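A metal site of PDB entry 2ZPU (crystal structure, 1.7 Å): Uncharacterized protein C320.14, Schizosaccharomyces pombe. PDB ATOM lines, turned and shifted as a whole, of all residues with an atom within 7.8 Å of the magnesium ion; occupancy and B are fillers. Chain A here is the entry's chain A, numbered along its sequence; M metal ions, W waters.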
ATOM      1  N   LEU A 182      11.557   2.900 -23.622  1.00  0.00           N
ATOM      2  CA  LEU A 182      11.631   4.298 -23.188  1.00  0.00           C
ATOM      3  C   LEU A 182      10.311   5.063 -23.023  1.00  0.00           C
ATOM      4  O   LEU A 182       9.562   5.235 -23.981  1.00  0.00           O
ATOM      5  CB  LEU A 182      12.525   5.105 -24.140  1.00  0.00           C
ATOM      6  CG  LEU A 182      12.610   6.616 -23.914  1.00  0.00           C
ATOM      7  CD1 LEU A 182      13.174   6.905 -22.524  1.00  0.00           C
ATOM      8  CD2 LEU A 182      13.499   7.252 -24.974  1.00  0.00           C
ATOM      9  N   GLY A 183      10.064   5.502 -21.801  1.00  0.00           N
ATOM     10  CA  GLY A 183       8.897   6.304 -21.479  1.00  0.00           C
ATOM     11  C   GLY A 183       9.495   7.627 -21.005  1.00  0.00           C
ATOM     12  O   GLY A 183       9.899   8.449 -21.819  1.00  0.00           O
ATOM     13  N   GLY A 184       9.568   7.801 -19.689  1.00  0.00           N
ATOM     14  CA  GLY A 184      10.144   9.010 -19.119  1.00  0.00           C
ATOM     15  C   GLY A 184      11.662   9.006 -19.086  1.00  0.00           C
ATOM     16  O   GLY A 184      12.291  10.059 -18.907  1.00  0.00           O
ATOM     17  N   VAL A 207      14.023   2.843 -27.009  1.00  0.00           N
ATOM     18  CA  VAL A 207      12.954   2.582 -27.986  1.00  0.00           C
ATOM     19  C   VAL A 207      11.612   3.100 -27.501  1.00  0.00           C
ATOM     20  O   VAL A 207      11.159   2.751 -26.406  1.00  0.00           O
ATOM     21  CB  VAL A 207      12.781   1.072 -28.263  1.00  0.00           C
ATOM     22  CG1 VAL A 207      11.815   0.872 -29.442  1.00  0.00           C
ATOM     23  CG2 VAL A 207      14.125   0.439 -28.567  1.00  0.00           C
ATOM     24  N   GLU A 208      10.949   3.914 -28.324  1.00  0.00           N
ATOM     25  CA  GLU A 208       9.646   4.462 -27.970  1.00  0.00           C
ATOM     26  C   GLU A 208       8.600   4.054 -28.995  1.00  0.00           C
ATOM     27  O   GLU A 208       8.930   3.678 -30.116  1.00  0.00           O
ATOM     28  CB  GLU A 208       9.672   5.992 -27.997  1.00  0.00           C
ATOM     29  CG  GLU A 208      10.614   6.666 -27.044  1.00  0.00           C
ATOM     30  CD  GLU A 208      10.559   8.164 -27.209  1.00  0.00           C
ATOM     31  OE1 GLU A 208      10.982   8.671 -28.265  1.00  0.00           O
ATOM     32  OE2 GLU A 208      10.074   8.846 -26.287  1.00  0.00           O
ATOM     33  N   PRO A 209       7.311   4.114 -28.618  1.00  0.00           N
ATOM     34  CA  PRO A 209       6.289   3.768 -29.603  1.00  0.00           C
ATOM     35  C   PRO A 209       6.352   4.940 -30.575  1.00  0.00           C
ATOM     36  O   PRO A 209       6.644   6.068 -30.161  1.00  0.00           O
ATOM     37  CB  PRO A 209       5.001   3.743 -28.773  1.00  0.00           C
ATOM     38  CG  PRO A 209       5.291   4.691 -27.643  1.00  0.00           C
ATOM     39  CD  PRO A 209       6.716   4.352 -27.291  1.00  0.00           C
ATOM     40  N   GLU A 210       6.116   4.700 -31.858  1.00  0.00           N
ATOM     41  CA  GLU A 210       6.205   5.779 -32.844  1.00  0.00           C
ATOM     42  C   GLU A 210       5.361   7.004 -32.558  1.00  0.00           C
ATOM     43  O   GLU A 210       5.808   8.140 -32.790  1.00  0.00           O
ATOM     44  CB  GLU A 210       5.895   5.255 -34.245  1.00  0.00           C
ATOM     45  CG  GLU A 210       4.650   4.401 -34.362  1.00  0.00           C
ATOM     46  CD  GLU A 210       4.421   3.951 -35.788  1.00  0.00           C
ATOM     47  OE1 GLU A 210       5.428   3.722 -36.505  1.00  0.00           O
ATOM     48  OE2 GLU A 210       3.248   3.828 -36.194  1.00  0.00           O
ATOM     49  N   ALA A 211       4.146   6.798 -32.074  1.00  0.00           N
ATOM     50  CA  ALA A 211       3.248   7.905 -31.764  1.00  0.00           C
ATOM     51  C   ALA A 211       3.769   8.768 -30.622  1.00  0.00           C
ATOM     52  O   ALA A 211       3.420   9.933 -30.497  1.00  0.00           O
ATOM     53  CB  ALA A 211       1.864   7.370 -31.429  1.00  0.00           C
ATOM     54  N   GLY A 212       4.616   8.175 -29.782  1.00  0.00           N
ATOM     55  CA  GLY A 212       5.168   8.928 -28.667  1.00  0.00           C
ATOM     56  C   GLY A 212       6.671   9.078 -28.779  1.00  0.00           C
ATOM     57  O   GLY A 212       7.383   8.757 -27.835  1.00  0.00           O
ATOM     58  N   ASN A 213       7.163   9.569 -29.906  1.00  0.00           N
ATOM     59  CA  ASN A 213       8.608   9.705 -30.084  1.00  0.00           C
ATOM     60  C   ASN A 213       9.205  11.026 -29.586  1.00  0.00           C
ATOM     61  O   ASN A 213      10.167  11.540 -30.167  1.00  0.00           O
ATOM     62  CB  ASN A 213       8.988   9.486 -31.563  1.00  0.00           C
ATOM     63  CG  ASN A 213       8.569  10.646 -32.465  1.00  0.00           C
ATOM     64  OD1 ASN A 213       9.091  10.799 -33.576  1.00  0.00           O
ATOM     65  ND2 ASN A 213       7.634  11.454 -31.997  1.00  0.00           N
ATOM     66  N   ASP A 214       8.656  11.565 -28.498  1.00  0.00           N
ATOM     67  CA  ASP A 214       9.159  12.810 -27.930  1.00  0.00           C
ATOM     68  C   ASP A 214      10.621  12.651 -27.507  1.00  0.00           C
ATOM     69  O   ASP A 214      11.438  13.556 -27.689  1.00  0.00           O
ATOM     70  CB  ASP A 214       8.338  13.222 -26.706  1.00  0.00           C
ATOM     71  CG  ASP A 214       8.258  12.133 -25.675  1.00  0.00           C
ATOM     72  OD1 ASP A 214       7.609  11.121 -25.979  1.00  0.00           O
ATOM     73  OD2 ASP A 214       8.842  12.275 -24.587  1.00  0.00           O
ATOM     74  N   GLY A 215      10.954  11.489 -26.943  1.00  0.00           N
ATOM     75  CA  GLY A 215      12.318  11.232 -26.514  1.00  0.00           C
ATOM     76  C   GLY A 215      13.281  11.246 -27.686  1.00  0.00           C
ATOM     77  O   GLY A 215      14.394  11.782 -27.587  1.00  0.00           O
ATOM     78  N   GLN A 216      12.855  10.664 -28.795  1.00  0.00           N
ATOM     79  CA  GLN A 216      13.686  10.614 -29.993  1.00  0.00           C
ATOM     80  C   GLN A 216      13.921  12.037 -30.499  1.00  0.00           C
ATOM     81  O   GLN A 216      15.038  12.401 -30.852  1.00  0.00           O
ATOM     82  CB  GLN A 216      12.985   9.799 -31.081  1.00  0.00           C
ATOM     83  CG  GLN A 216      13.808   9.574 -32.339  1.00  0.00           C
ATOM     84  CD  GLN A 216      13.036   8.780 -33.373  1.00  0.00           C
ATOM     85  OE1 GLN A 216      11.976   9.213 -33.829  1.00  0.00           O
ATOM     86  NE2 GLN A 216      13.550   7.613 -33.750  1.00  0.00           N
ATOM     87  N   VAL A 225      11.582  17.860 -25.812  1.00  0.00           N
ATOM     88  CA  VAL A 225      10.470  18.112 -26.706  1.00  0.00           C
ATOM     89  C   VAL A 225       9.204  17.605 -26.020  1.00  0.00           C
ATOM     90  O   VAL A 225       9.203  16.503 -25.453  1.00  0.00           O
ATOM     91  CB  VAL A 225      10.647  17.385 -28.054  1.00  0.00           C
ATOM     92  CG1 VAL A 225       9.383  17.523 -28.909  1.00  0.00           C
ATOM     93  CG2 VAL A 225      11.842  17.972 -28.799  1.00  0.00           C
ATOM     94  N   ILE A 227       5.082  16.637 -26.239  1.00  0.00           N
ATOM     95  CA  ILE A 227       4.026  16.238 -27.152  1.00  0.00           C
ATOM     96  C   ILE A 227       2.738  15.989 -26.390  1.00  0.00           C
ATOM     97  O   ILE A 227       2.741  15.854 -25.165  1.00  0.00           O
ATOM     98  CB  ILE A 227       4.395  14.931 -27.907  1.00  0.00           C
ATOM     99  CG1 ILE A 227       4.482  13.759 -26.917  1.00  0.00           C
ATOM    100  CG2 ILE A 227       5.716  15.125 -28.639  1.00  0.00           C
ATOM    101  CD1 ILE A 227       4.647  12.399 -27.579  1.00  0.00           C
ATOM    102  N   PRO A 230       0.406  10.582 -26.314  1.00  0.00           N
ATOM    103  CA  PRO A 230       0.233   9.739 -27.506  1.00  0.00           C
ATOM    104  C   PRO A 230      -0.715   8.562 -27.306  1.00  0.00           C
ATOM    105  O   PRO A 230      -0.801   7.997 -26.216  1.00  0.00           O
ATOM    106  CB  PRO A 230       1.660   9.276 -27.787  1.00  0.00           C
ATOM    107  CG  PRO A 230       2.180   9.055 -26.400  1.00  0.00           C
ATOM    108  CD  PRO A 230       1.698  10.304 -25.666  1.00  0.00           C
ATOM    109  N   ALA A 237       4.462   3.879 -21.799  1.00  0.00           N
ATOM    110  CA  ALA A 237       5.344   4.773 -22.548  1.00  0.00           C
ATOM    111  C   ALA A 237       4.605   5.970 -23.152  1.00  0.00           C
ATOM    112  O   ALA A 237       5.069   6.569 -24.128  1.00  0.00           O
ATOM    113  CB  ALA A 237       6.064   3.982 -23.649  1.00  0.00           C
ATOM    114  N   GLN A 238       3.463   6.317 -22.578  1.00  0.00           N
ATOM    115  CA  GLN A 238       2.656   7.418 -23.079  1.00  0.00           C
ATOM    116  C   GLN A 238       2.997   8.776 -22.471  1.00  0.00           C
ATOM    117  O   GLN A 238       2.156   9.683 -22.419  1.00  0.00           O
ATOM    118  CB  GLN A 238       1.175   7.120 -22.859  1.00  0.00           C
ATOM    119  CG  GLN A 238       0.623   6.072 -23.800  1.00  0.00           C
ATOM    120  CD  GLN A 238      -0.812   5.697 -23.472  1.00  0.00           C
ATOM    121  OE1 GLN A 238      -1.057   4.845 -22.621  1.00  0.00           O
ATOM    122  NE2 GLN A 238      -1.759   6.349 -24.146  1.00  0.00           N
ATOM    123  N   THR A 239       4.243   8.910 -22.026  1.00  0.00           N
ATOM    124  CA  THR A 239       4.722  10.145 -21.415  1.00  0.00           C
ATOM    125  C   THR A 239       4.783  11.289 -22.435  1.00  0.00           C
ATOM    126  O   THR A 239       5.041  11.062 -23.614  1.00  0.00           O
ATOM    127  CB  THR A 239       6.130   9.924 -20.841  1.00  0.00           C
ATOM    128  OG1 THR A 239       6.824   8.960 -21.637  1.00  0.00           O
ATOM    129  CG2 THR A 239       6.044   9.427 -19.401  1.00  0.00           C
ATOM    130  N   GLN A 240       4.529  12.510 -21.971  1.00  0.00           N
ATOM    131  CA  GLN A 240       4.546  13.683 -22.856  1.00  0.00           C
ATOM    132  C   GLN A 240       5.952  14.209 -23.104  1.00  0.00           C
ATOM    133  O   GLN A 240       6.210  14.882 -24.099  1.00  0.00           O
ATOM    134  CB  GLN A 240       3.655  14.784 -22.274  1.00  0.00           C
ATOM    135  CG  GLN A 240       2.200  14.369 -22.140  1.00  0.00           C
ATOM    136  CD  GLN A 240       1.289  15.504 -21.729  1.00  0.00           C
ATOM    137  OE1 GLN A 240       0.084  15.319 -21.589  1.00  0.00           O
ATOM    138  NE2 GLN A 240       1.859  16.690 -21.547  1.00  0.00           N
ATOM    139  N   HIS A 241       6.860  13.914 -22.182  1.00  0.00           N
ATOM    140  CA  HIS A 241       8.243  14.351 -22.324  1.00  0.00           C
ATOM    141  C   HIS A 241       9.171  13.633 -21.349  1.00  0.00           C
ATOM    142  O   HIS A 241       8.719  13.028 -20.376  1.00  0.00           O
ATOM    143  CB  HIS A 241       8.339  15.877 -22.136  1.00  0.00           C
ATOM    144  CG  HIS A 241       7.982  16.342 -20.759  1.00  0.00           C
ATOM    145  ND1 HIS A 241       8.868  16.268 -19.706  1.00  0.00           N
ATOM    146  CD2 HIS A 241       6.844  16.881 -20.268  1.00  0.00           C
ATOM    147  CE1 HIS A 241       8.285  16.743 -18.614  1.00  0.00           C
ATOM    148  NE2 HIS A 241       7.058  17.118 -18.922  1.00  0.00           N
ATOM    149  N   LEU A 242      10.464  13.695 -21.629  1.00  0.00           N
ATOM    150  CA  LEU A 242      11.460  13.053 -20.783  1.00  0.00           C
ATOM    151  C   LEU A 242      11.689  13.832 -19.499  1.00  0.00           C
ATOM    152  O   LEU A 242      11.419  15.030 -19.427  1.00  0.00           O
ATOM    153  CB  LEU A 242      12.785  12.927 -21.532  1.00  0.00           C
ATOM    154  CG  LEU A 242      12.842  12.064 -22.781  1.00  0.00           C
ATOM    155  CD1 LEU A 242      14.246  12.113 -23.367  1.00  0.00           C
ATOM    156  CD2 LEU A 242      12.460  10.635 -22.433  1.00  0.00           C
ATOM    157  N   ILE A 257      17.846   6.618 -30.383  1.00  0.00           N
ATOM    158  CA  ILE A 257      16.493   6.311 -29.909  1.00  0.00           C
ATOM    159  C   ILE A 257      15.717   5.851 -31.137  1.00  0.00           C
ATOM    160  O   ILE A 257      15.664   6.550 -32.139  1.00  0.00           O
ATOM    161  CB  ILE A 257      15.776   7.558 -29.312  1.00  0.00           C
ATOM    162  CG1 ILE A 257      16.602   8.157 -28.180  1.00  0.00           C
ATOM    163  CG2 ILE A 257      14.390   7.152 -28.803  1.00  0.00           C
ATOM    164  CD1 ILE A 257      16.823   7.229 -27.001  1.00  0.00           C
ATOM    165  N   THR A 259      12.063   3.792 -32.850  1.00  0.00           N
ATOM    166  CA  THR A 259      10.625   3.695 -32.652  1.00  0.00           C
ATOM    167  C   THR A 259      10.100   2.492 -33.407  1.00  0.00           C
ATOM    168  O   THR A 259      10.718   2.035 -34.385  1.00  0.00           O
ATOM    169  CB  THR A 259       9.849   4.947 -33.167  1.00  0.00           C
ATOM    170  OG1 THR A 259      10.002   5.060 -34.589  1.00  0.00           O
ATOM    171  CG2 THR A 259      10.341   6.214 -32.483  1.00  0.00           C
HETATM  172 MG    MG M   1       7.934   9.028 -25.660  1.00  0.00          MG
HETATM  173  O   HOH W   1       8.568   9.792 -23.648  1.00  0.00           O
HETATM  174  O   HOH W   2       7.787   6.937 -25.067  1.00  0.00           O
HETATM  175  O   HOH W   3       5.728   9.013 -25.119  1.00  0.00           O
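Within 4 Å of the magnesium ion: Glu 208, Gly 212 and Asp 214.
OE1 of Glu 208 is in hydrogen-bond range of N of Gly 215, 3.1 Å away. The backbone NH (N) of Gln 216 is in hydrogen-bond range of the side-chain carboxylate (OE1) of Glu 208 (2.8 Å).
OD1 of Asp 214 binds the magnesium ion (2.1 Å). Water W2 is bound to the magnesium ion (2.2 Å). The side-chain carboxylate (OE2) of Glu 208 binds the magnesium ion, 2.2 Å away. The magnesium ion is bound by water W1 (2.2 Å). The magnesium ion is bound by O of Gly 212, at 2.3 Å. Water W3 binds the magnesium ion. The magnesium ion has six donor atoms within binding distance.
Water W1 lies within hydrogen-bond range of the backbone carbonyl oxygen of Gly 183, the side-chain carboxylate of Asp 214 and the side-chain hydroxyl of Thr 239. Water W2 lies within hydrogen-bond range of O of Leu 182 (2.7 Å) and O of Ala 237 (2.9 Å).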
